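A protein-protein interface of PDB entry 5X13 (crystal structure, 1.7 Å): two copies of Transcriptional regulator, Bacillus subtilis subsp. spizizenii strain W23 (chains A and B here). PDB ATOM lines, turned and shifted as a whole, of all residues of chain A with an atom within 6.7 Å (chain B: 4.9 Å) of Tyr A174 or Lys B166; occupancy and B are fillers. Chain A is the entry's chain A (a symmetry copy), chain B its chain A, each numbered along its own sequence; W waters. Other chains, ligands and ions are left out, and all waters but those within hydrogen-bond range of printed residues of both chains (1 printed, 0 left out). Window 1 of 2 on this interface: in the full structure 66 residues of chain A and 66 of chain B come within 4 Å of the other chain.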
ATOM      1  N   ASP A 102     -23.923   9.884  19.808  1.00  0.00           N
ATOM      2  CA  ASP A 102     -24.913   8.785  19.742  1.00  0.00           C
ATOM      3  C   ASP A 102     -24.145   7.521  20.101  1.00  0.00           C
ATOM      4  O   ASP A 102     -23.304   7.056  19.340  1.00  0.00           O
ATOM      5  CB  ASP A 102     -25.502   8.748  18.349  1.00  0.00           C
ATOM      6  CG  ASP A 102     -26.557   7.655  18.172  1.00  0.00           C
ATOM      7  OD1 ASP A 102     -26.515   6.645  18.915  1.00  0.00           O
ATOM      8  OD2 ASP A 102     -27.354   7.834  17.239  1.00  0.00           O
ATOM      9  N   GLU A 103     -24.389   6.987  21.304  1.00  0.00           N
ATOM     10  CA  GLU A 103     -23.631   5.839  21.781  1.00  0.00           C
ATOM     11  C   GLU A 103     -23.780   4.628  20.888  1.00  0.00           C
ATOM     12  O   GLU A 103     -22.839   3.865  20.706  1.00  0.00           O
ATOM     13  CB  GLU A 103     -24.030   5.492  23.207  1.00  0.00           C
ATOM     14  CG  GLU A 103     -22.924   4.895  24.038  1.00  0.00           C
ATOM     15  CD  GLU A 103     -23.408   4.664  25.459  1.00  0.00           C
ATOM     16  OE1 GLU A 103     -24.416   5.298  25.843  1.00  0.00           O
ATOM     17  OE2 GLU A 103     -22.825   3.815  26.169  1.00  0.00           O
ATOM     18  N   PHE A 104     -24.962   4.456  20.292  1.00  0.00           N
ATOM     19  CA  PHE A 104     -25.135   3.368  19.363  1.00  0.00           C
ATOM     20  C   PHE A 104     -24.160   3.461  18.206  1.00  0.00           C
ATOM     21  O   PHE A 104     -23.649   2.462  17.722  1.00  0.00           O
ATOM     22  CB  PHE A 104     -26.588   3.295  18.819  1.00  0.00           C
ATOM     23  CG  PHE A 104     -26.774   2.211  17.811  1.00  0.00           C
ATOM     24  CD1 PHE A 104     -26.968   0.901  18.175  1.00  0.00           C
ATOM     25  CD2 PHE A 104     -26.749   2.497  16.470  1.00  0.00           C
ATOM     26  CE1 PHE A 104     -27.101  -0.085  17.220  1.00  0.00           C
ATOM     27  CE2 PHE A 104     -26.880   1.534  15.539  1.00  0.00           C
ATOM     28  CZ  PHE A 104     -27.064   0.241  15.899  1.00  0.00           C
ATOM     29  N   MET A 105     -23.947   4.675  17.738  1.00  0.00           N
ATOM     30  CA  MET A 105     -23.081   4.918  16.566  1.00  0.00           C
ATOM     31  C   MET A 105     -21.630   4.674  16.913  1.00  0.00           C
ATOM     32  O   MET A 105     -20.885   4.202  16.055  1.00  0.00           O
ATOM     33  CB  MET A 105     -23.319   6.318  15.965  1.00  0.00           C
ATOM     34  CG  MET A 105     -24.776   6.354  15.264  1.00  0.00           C
ATOM     35  SD  MET A 105     -25.017   5.087  14.102  1.00  0.00           S
ATOM     36  CE  MET A 105     -23.544   5.255  13.019  1.00  0.00           C
ATOM     37  N   GLN A 126     -31.849  -2.151  17.890  1.00  0.00           N
ATOM     38  CA  GLN A 126     -31.948  -0.744  17.659  1.00  0.00           C
ATOM     39  C   GLN A 126     -33.113  -0.433  16.706  1.00  0.00           C
ATOM     40  O   GLN A 126     -33.874   0.493  16.921  1.00  0.00           O
ATOM     41  CB  GLN A 126     -30.639  -0.207  17.166  1.00  0.00           C
ATOM     42  CG  GLN A 126     -30.562   1.344  17.110  1.00  0.00           C
ATOM     43  CD  GLN A 126     -30.540   2.056  18.488  1.00  0.00           C
ATOM     44  OE1 GLN A 126     -30.680   3.273  18.532  1.00  0.00           O
ATOM     45  NE2 GLN A 126     -30.271   1.328  19.564  1.00  0.00           N
ATOM     46  N   LEU A 127     -33.261  -1.221  15.654  1.00  0.00           N
ATOM     47  CA  LEU A 127     -34.348  -1.017  14.692  1.00  0.00           C
ATOM     48  C   LEU A 127     -35.704  -1.125  15.392  1.00  0.00           C
ATOM     49  O   LEU A 127     -36.603  -0.297  15.180  1.00  0.00           O
ATOM     50  CB  LEU A 127     -34.283  -2.065  13.588  1.00  0.00           C
ATOM     51  CG  LEU A 127     -35.471  -2.047  12.630  1.00  0.00           C
ATOM     52  CD1 LEU A 127     -35.323  -0.841  11.672  1.00  0.00           C
ATOM     53  CD2 LEU A 127     -35.624  -3.379  11.955  1.00  0.00           C
ATOM     54  N   ARG A 130     -36.338   1.952  17.475  1.00  0.00           N
ATOM     55  CA  ARG A 130     -36.578   3.144  16.661  1.00  0.00           C
ATOM     56  C   ARG A 130     -37.955   3.072  15.968  1.00  0.00           C
ATOM     57  O   ARG A 130     -38.617   4.089  15.817  1.00  0.00           O
ATOM     58  CB  ARG A 130     -35.462   3.334  15.629  1.00  0.00           C
ATOM     59  CG  ARG A 130     -34.049   3.596  16.257  1.00  0.00           C
ATOM     60  CD  ARG A 130     -33.678   5.000  16.363  1.00  0.00           C
ATOM     61  NE  ARG A 130     -32.527   5.224  17.241  1.00  0.00           N
ATOM     62  CZ  ARG A 130     -32.325   6.384  17.844  1.00  0.00           C
ATOM     63  NH1 ARG A 130     -33.220   7.354  17.668  1.00  0.00           N
ATOM     64  NH2 ARG A 130     -31.265   6.555  18.657  1.00  0.00           N
ATOM     65  N   GLU A 169     -39.330  12.622  10.438  1.00  0.00           N
ATOM     66  CA  GLU A 169     -38.343  12.451   9.359  1.00  0.00           C
ATOM     67  C   GLU A 169     -37.052  11.885   9.891  1.00  0.00           C
ATOM     68  O   GLU A 169     -36.462  10.997   9.301  1.00  0.00           O
ATOM     69  CB  GLU A 169     -38.049  13.793   8.702  1.00  0.00           C
ATOM     70  CG  GLU A 169     -39.105  14.148   7.687  1.00  0.00           C
ATOM     71  CD  GLU A 169     -39.212  13.118   6.556  1.00  0.00           C
ATOM     72  OE1 GLU A 169     -38.214  12.923   5.831  1.00  0.00           O
ATOM     73  OE2 GLU A 169     -40.296  12.503   6.406  1.00  0.00           O
ATOM     74  N   ARG A 170     -36.611  12.422  11.036  1.00  0.00           N
ATOM     75  CA  ARG A 170     -35.367  12.008  11.666  1.00  0.00           C
ATOM     76  C   ARG A 170     -35.403  10.507  11.995  1.00  0.00           C
ATOM     77  O   ARG A 170     -34.470   9.745  11.692  1.00  0.00           O
ATOM     78  CB  ARG A 170     -35.145  12.783  12.960  1.00  0.00           C
ATOM     79  CG  ARG A 170     -33.894  12.443  13.706  1.00  0.00           C
ATOM     80  CD  ARG A 170     -33.829  13.225  15.101  1.00  0.00           C
ATOM     81  NE  ARG A 170     -34.797  12.580  15.971  1.00  0.00           N
ATOM     82  CZ  ARG A 170     -35.706  13.169  16.747  1.00  0.00           C
ATOM     83  NH1 ARG A 170     -35.796  14.477  16.861  1.00  0.00           N
ATOM     84  NH2 ARG A 170     -36.539  12.410  17.439  1.00  0.00           N
ATOM     85  N   GLU A 171     -36.475  10.093  12.638  1.00  0.00           N
ATOM     86  CA  GLU A 171     -36.594   8.698  13.047  1.00  0.00           C
ATOM     87  C   GLU A 171     -36.865   7.779  11.861  1.00  0.00           C
ATOM     88  O   GLU A 171     -36.317   6.691  11.806  1.00  0.00           O
ATOM     89  CB  GLU A 171     -37.637   8.499  14.131  1.00  0.00           C
ATOM     90  CG  GLU A 171     -37.338   9.196  15.440  1.00  0.00           C
ATOM     91  CD  GLU A 171     -35.966   8.870  16.043  1.00  0.00           C
ATOM     92  OE1 GLU A 171     -35.446   7.732  15.865  1.00  0.00           O
ATOM     93  OE2 GLU A 171     -35.421   9.767  16.714  1.00  0.00           O
ATOM     94  N   LYS A 172     -37.688   8.192  10.891  1.00  0.00           N
ATOM     95  CA  LYS A 172     -37.858   7.387   9.647  1.00  0.00           C
ATOM     96  C   LYS A 172     -36.525   7.148   8.952  1.00  0.00           C
ATOM     97  O   LYS A 172     -36.209   6.059   8.492  1.00  0.00           O
ATOM     98  CB  LYS A 172     -38.797   8.105   8.715  1.00  0.00           C
ATOM     99  CG  LYS A 172     -40.228   8.030   9.092  1.00  0.00           C
ATOM    100  CD  LYS A 172     -41.081   8.942   8.229  1.00  0.00           C
ATOM    101  CE  LYS A 172     -42.573   8.900   8.626  1.00  0.00           C
ATOM    102  NZ  LYS A 172     -43.402   9.795   7.704  1.00  0.00           N
ATOM    103  N   ASN A 173     -35.718   8.197   8.866  1.00  0.00           N
ATOM    104  CA  ASN A 173     -34.398   8.085   8.259  1.00  0.00           C
ATOM    105  C   ASN A 173     -33.465   7.144   9.030  1.00  0.00           C
ATOM    106  O   ASN A 173     -32.741   6.319   8.406  1.00  0.00           O
ATOM    107  CB  ASN A 173     -33.771   9.476   8.108  1.00  0.00           C
ATOM    108  CG  ASN A 173     -32.419   9.448   7.371  1.00  0.00           C
ATOM    109  OD1 ASN A 173     -31.334   9.518   7.987  1.00  0.00           O
ATOM    110  ND2 ASN A 173     -32.492   9.279   6.089  1.00  0.00           N
ATOM    111  N   TYR A 174     -33.522   7.187  10.342  1.00  0.00           N
ATOM    112  CA  TYR A 174     -32.723   6.305  11.183  1.00  0.00           C
ATOM    113  C   TYR A 174     -33.149   4.869  10.923  1.00  0.00           C
ATOM    114  O   TYR A 174     -32.308   3.954  10.823  1.00  0.00           O
ATOM    115  CB  TYR A 174     -32.855   6.678  12.679  1.00  0.00           C
ATOM    116  CG  TYR A 174     -31.634   6.411  13.559  1.00  0.00           C
ATOM    117  CD1 TYR A 174     -31.030   5.152  13.615  1.00  0.00           C
ATOM    118  CD2 TYR A 174     -31.175   7.382  14.447  1.00  0.00           C
ATOM    119  CE1 TYR A 174     -29.957   4.892  14.457  1.00  0.00           C
ATOM    120  CE2 TYR A 174     -30.104   7.113  15.305  1.00  0.00           C
ATOM    121  CZ  TYR A 174     -29.507   5.866  15.315  1.00  0.00           C
ATOM    122  OH  TYR A 174     -28.436   5.634  16.166  1.00  0.00           O
ATOM    123  N   VAL A 175     -34.457   4.643  10.870  1.00  0.00           N
ATOM    124  CA  VAL A 175     -34.991   3.320  10.617  1.00  0.00           C
ATOM    125  C   VAL A 175     -34.548   2.835   9.253  1.00  0.00           C
ATOM    126  O   VAL A 175     -34.105   1.685   9.117  1.00  0.00           O
ATOM    127  CB  VAL A 175     -36.540   3.312  10.740  1.00  0.00           C
ATOM    128  CG1 VAL A 175     -37.190   2.036  10.133  1.00  0.00           C
ATOM    129  CG2 VAL A 175     -36.934   3.408  12.226  1.00  0.00           C
ATOM    130  N   SER A 176     -34.645   3.679   8.239  1.00  0.00           N
ATOM    131  CA  SER A 176     -34.243   3.235   6.894  1.00  0.00           C
ATOM    132  C   SER A 176     -32.761   2.897   6.826  1.00  0.00           C
ATOM    133  O   SER A 176     -32.377   1.925   6.153  1.00  0.00           O
ATOM    134  CB  SER A 176     -34.578   4.297   5.854  1.00  0.00           C
ATOM    135  OG  SER A 176     -35.962   4.403   5.699  1.00  0.00           O
ATOM    136  N   TRP A 177     -31.927   3.681   7.488  1.00  0.00           N
ATOM    137  CA  TRP A 177     -30.520   3.414   7.546  1.00  0.00           C
ATOM    138  C   TRP A 177     -30.248   2.075   8.256  1.00  0.00           C
ATOM    139  O   TRP A 177     -29.466   1.246   7.778  1.00  0.00           O
ATOM    140  CB  TRP A 177     -29.775   4.569   8.237  1.00  0.00           C
ATOM    141  CG  TRP A 177     -28.317   4.312   8.353  1.00  0.00           C
ATOM    142  CD1 TRP A 177     -27.345   4.539   7.406  1.00  0.00           C
ATOM    143  CD2 TRP A 177     -27.640   3.836   9.503  1.00  0.00           C
ATOM    144  NE1 TRP A 177     -26.120   4.177   7.898  1.00  0.00           N
ATOM    145  CE2 TRP A 177     -26.265   3.733   9.175  1.00  0.00           C
ATOM    146  CE3 TRP A 177     -28.059   3.428  10.769  1.00  0.00           C
ATOM    147  CZ2 TRP A 177     -25.311   3.293  10.087  1.00  0.00           C
ATOM    148  CZ3 TRP A 177     -27.102   3.001  11.682  1.00  0.00           C
ATOM    149  CH2 TRP A 177     -25.751   2.930  11.345  1.00  0.00           C
ATOM    150  N   LEU A 178     -30.889   1.852   9.393  1.00  0.00           N
ATOM    151  CA  LEU A 178     -30.703   0.571  10.068  1.00  0.00           C
ATOM    152  C   LEU A 178     -31.121  -0.603   9.183  1.00  0.00           C
ATOM    153  O   LEU A 178     -30.481  -1.659   9.178  1.00  0.00           O
ATOM    154  CB  LEU A 178     -31.491   0.506  11.364  1.00  0.00           C
ATOM    155  CG  LEU A 178     -31.006   1.404  12.478  1.00  0.00           C
ATOM    156  CD1 LEU A 178     -32.087   1.631  13.551  1.00  0.00           C
ATOM    157  CD2 LEU A 178     -29.715   0.873  13.113  1.00  0.00           C
ATOM    158  N   GLU A 179     -32.240  -0.463   8.473  1.00  0.00           N
ATOM    159  CA  GLU A 179     -32.682  -1.510   7.550  1.00  0.00           C
ATOM    160  C   GLU A 179     -31.584  -1.783   6.494  1.00  0.00           C
ATOM    161  O   GLU A 179     -31.294  -2.957   6.162  1.00  0.00           O
ATOM    162  CB  GLU A 179     -34.005  -1.098   6.870  1.00  0.00           C
ATOM    163  CG  GLU A 179     -35.159  -1.092   7.858  1.00  0.00           C
ATOM    164  CD  GLU A 179     -36.477  -0.595   7.300  1.00  0.00           C
ATOM    165  OE1 GLU A 179     -36.444   0.098   6.295  1.00  0.00           O
ATOM    166  OE2 GLU A 179     -37.501  -0.851   7.995  1.00  0.00           O
ATOM    167  N   TYR B 161     -17.415   3.211   7.592  1.00  0.00           N
ATOM    168  CA  TYR B 161     -18.543   3.330   6.634  1.00  0.00           C
ATOM    169  C   TYR B 161     -19.866   3.554   7.320  1.00  0.00           C
ATOM    170  O   TYR B 161     -20.679   4.391   6.911  1.00  0.00           O
ATOM    171  CB  TYR B 161     -18.536   2.102   5.733  1.00  0.00           C
ATOM    172  CG  TYR B 161     -19.674   2.001   4.760  1.00  0.00           C
ATOM    173  CD1 TYR B 161     -19.598   2.583   3.537  1.00  0.00           C
ATOM    174  CD2 TYR B 161     -20.784   1.259   5.041  1.00  0.00           C
ATOM    175  CE1 TYR B 161     -20.604   2.479   2.589  1.00  0.00           C
ATOM    176  CE2 TYR B 161     -21.803   1.131   4.103  1.00  0.00           C
ATOM    177  CZ  TYR B 161     -21.698   1.703   2.888  1.00  0.00           C
ATOM    178  OH  TYR B 161     -22.696   1.631   1.929  1.00  0.00           O
ATOM    179  N   LEU B 162     -20.097   2.835   8.412  1.00  0.00           N
ATOM    180  CA  LEU B 162     -21.351   2.974   9.149  1.00  0.00           C
ATOM    181  C   LEU B 162     -21.494   4.385   9.702  1.00  0.00           C
ATOM    182  O   LEU B 162     -22.520   4.998   9.519  1.00  0.00           O
ATOM    183  CB  LEU B 162     -21.481   1.921  10.272  1.00  0.00           C
ATOM    184  CG  LEU B 162     -21.547   0.454   9.822  1.00  0.00           C
ATOM    185  CD1 LEU B 162     -21.750  -0.426  11.077  1.00  0.00           C
ATOM    186  CD2 LEU B 162     -22.659   0.238   8.741  1.00  0.00           C
ATOM    187  N   VAL B 163     -20.467   4.924  10.354  1.00  0.00           N
ATOM    188  CA  VAL B 163     -20.619   6.257  10.972  1.00  0.00           C
ATOM    189  C   VAL B 163     -20.753   7.336   9.872  1.00  0.00           C
ATOM    190  O   VAL B 163     -21.497   8.277  10.070  1.00  0.00           O
ATOM    191  CB  VAL B 163     -19.499   6.587  11.987  1.00  0.00           C
ATOM    192  CG1 VAL B 163     -19.601   5.667  13.155  1.00  0.00           C
ATOM    193  CG2 VAL B 163     -18.100   6.462  11.373  1.00  0.00           C
ATOM    194  N   LEU B 164     -20.056   7.156   8.761  1.00  0.00           N
ATOM    195  CA  LEU B 164     -20.113   8.131   7.693  1.00  0.00           C
ATOM    196  C   LEU B 164     -21.435   8.099   6.935  1.00  0.00           C
ATOM    197  O   LEU B 164     -22.009   9.154   6.678  1.00  0.00           O
ATOM    198  CB  LEU B 164     -18.951   8.003   6.738  1.00  0.00           C
ATOM    199  CG  LEU B 164     -18.814   9.148   5.745  1.00  0.00           C
ATOM    200  CD1 LEU B 164     -18.944  10.565   6.367  1.00  0.00           C
ATOM    201  CD2 LEU B 164     -17.474   8.993   5.159  1.00  0.00           C
ATOM    202  N   THR B 165     -21.936   6.912   6.611  1.00  0.00           N
ATOM    203  CA  THR B 165     -23.222   6.819   5.918  1.00  0.00           C
ATOM    204  C   THR B 165     -24.331   7.339   6.825  1.00  0.00           C
ATOM    205  O   THR B 165     -25.322   7.939   6.342  1.00  0.00           O
ATOM    206  CB  THR B 165     -23.503   5.438   5.370  1.00  0.00           C
ATOM    207  OG1 THR B 165     -23.497   4.462   6.425  1.00  0.00           O
ATOM    208  CG2 THR B 165     -22.466   5.009   4.303  1.00  0.00           C
ATOM    209  N   LYS B 166     -24.244   7.041   8.119  1.00  0.00           N
ATOM    210  CA  LYS B 166     -25.217   7.533   9.052  1.00  0.00           C
ATOM    211  C   LYS B 166     -25.274   9.077   8.973  1.00  0.00           C
ATOM    212  O   LYS B 166     -26.365   9.680   8.922  1.00  0.00           O
ATOM    213  CB  LYS B 166     -24.880   7.110  10.476  1.00  0.00           C
ATOM    214  CG  LYS B 166     -25.848   7.634  11.521  1.00  0.00           C
ATOM    215  CD  LYS B 166     -27.163   6.885  11.383  1.00  0.00           C
ATOM    216  CE  LYS B 166     -28.136   7.316  12.434  1.00  0.00           C
ATOM    217  NZ  LYS B 166     -28.969   8.423  11.947  1.00  0.00           N
ATOM    218  N   ALA B 167     -24.104   9.697   9.023  1.00  0.00           N
ATOM    219  CA  ALA B 167     -23.990  11.162   9.010  1.00  0.00           C
ATOM    220  C   ALA B 167     -24.512  11.788   7.713  1.00  0.00           C
ATOM    221  O   ALA B 167     -25.275  12.756   7.749  1.00  0.00           O
ATOM    222  CB  ALA B 167     -22.563  11.576   9.237  1.00  0.00           C
ATOM    223  N   LEU B 168     -24.171  11.153   6.607  1.00  0.00           N
ATOM    224  CA  LEU B 168     -24.622  11.565   5.275  1.00  0.00           C
ATOM    225  C   LEU B 168     -26.136  11.515   5.189  1.00  0.00           C
ATOM    226  O   LEU B 168     -26.771  12.505   4.822  1.00  0.00           O
ATOM    227  CB  LEU B 168     -24.044  10.658   4.198  1.00  0.00           C
ATOM    228  CG  LEU B 168     -22.629  10.852   3.841  1.00  0.00           C
ATOM    229  CD1 LEU B 168     -22.159   9.614   3.056  1.00  0.00           C
ATOM    230  CD2 LEU B 168     -22.462  12.198   3.021  1.00  0.00           C
ATOM    231  N   GLU B 169     -26.730  10.405   5.623  1.00  0.00           N
ATOM    232  CA  GLU B 169     -28.191  10.231   5.619  1.00  0.00           C
ATOM    233  C   GLU B 169     -28.861  11.249   6.504  1.00  0.00           C
ATOM    234  O   GLU B 169     -29.869  11.834   6.143  1.00  0.00           O
ATOM    235  CB  GLU B 169     -28.553   8.839   6.123  1.00  0.00           C
ATOM    236  CG  GLU B 169     -28.421   7.811   5.029  1.00  0.00           C
ATOM    237  CD  GLU B 169     -29.335   8.097   3.832  1.00  0.00           C
ATOM    238  OE1 GLU B 169     -30.570   8.119   4.015  1.00  0.00           O
ATOM    239  OE2 GLU B 169     -28.808   8.306   2.711  1.00  0.00           O
ATOM    240  N   ARG B 170     -28.280  11.457   7.693  1.00  0.00           N
ATOM    241  CA  ARG B 170     -28.818  12.386   8.675  1.00  0.00           C
ATOM    242  C   ARG B 170     -28.894  13.805   8.089  1.00  0.00           C
ATOM    243  O   ARG B 170     -29.920  14.499   8.179  1.00  0.00           O
ATOM    244  CB  ARG B 170     -27.930  12.420   9.914  1.00  0.00           C
ATOM    245  CG  ARG B 170     -28.377  13.346  11.000  1.00  0.00           C
ATOM    246  CD  ARG B 170     -27.309  13.389  12.191  1.00  0.00           C
ATOM    247  NE  ARG B 170     -26.178  14.153  11.692  1.00  0.00           N
ATOM    248  CZ  ARG B 170     -24.887  13.843  11.790  1.00  0.00           C
ATOM    249  NH1 ARG B 170     -24.463  12.778  12.437  1.00  0.00           N
ATOM    250  NH2 ARG B 170     -23.996  14.643  11.228  1.00  0.00           N
HETATM  251  O   HOH W   1     -31.418  10.848   3.847  1.00  0.00           O
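Hydrophobic or aromatic side chains of chain A within 4 Å of the printed part of chain B: Met A105, Tyr A174 and Trp A177. Hydrophobic or aromatic side chains of chain B that line the printed part of chain A: Val B163. Among the printed residues, 9 pairs touch across the chains. Among the printed residues, no Asp or Glu carboxylate lies within 4 Å of a Lys or Arg side-chain nitrogen of the other chain.
O of Tyr B161 lies within hydrogen-bond range of OG1 of Thr B165. O of Leu B162 is in hydrogen-bond range of OG1 of Thr B165 (3.3 Å). The side-chain carboxylate (OD1) of Asp A102 is in hydrogen-bond range of the backbone NH (N) of Met A105 (3.4 Å). The side-chain carboxylate (OD2) of Asp A102 sits at hydrogen-bond distance from the side-chain hydroxyl (OH) of Tyr A174 (2.7 Å).
Among the printed residues, merely in contact across the chains: Trp A177 with Leu B162 (3.3 Å), Met A105 with Lys B166 (3.4 Å), Tyr A174 with Lys B166 (3.5 Å), Met A105 with Val B163 (3.5 Å), Asn A173 with Arg B170 (3.6 Å) and Met A105 with Leu B162 (3.7 Å).
OG1 of Thr B165 is in hydrogen-bond range of NE1 of Trp A177 (3.0 Å). The side-chain amide nitrogen of Asn A173 is in hydrogen-bond range of the side-chain carboxylate of Glu B169 (3.1 Å). NE1 of Trp A177 sits close to N of Lys B166 (3.4 Å).
Water W1 bridges OE1 of Glu B169 (2.9 Å) and ND2 of Asn A173 (2.9 Å).
2 positions are printed for both chains. Of the 9 pairs that touch across the chains among the printed residues, none has its exchanged pair printed and touching as well.
Glu A169 touches none of the printed residues of chain B. Glu A171 touches none of the printed residues of chain B. Of the printed residues of chain B, Asn A173 touches Glu B169 and Arg B170. Of chain B, only Lys B166 comes within 4 Å of Tyr A174. Of the printed residues of chain A, Val B163 touches Met A105. Lys B166 touches just these residues of chain A: Met A105 (3.4 Å), Tyr A174 (3.5 Å) and Trp A177 (3.4 Å). The nearest printed residue of chain B that does not touch Tyr A174 is Glu B169 (6.7 Å). The nearest printed residue of chain A that does not touch Arg B170 is Arg A170 (6.2 Å).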
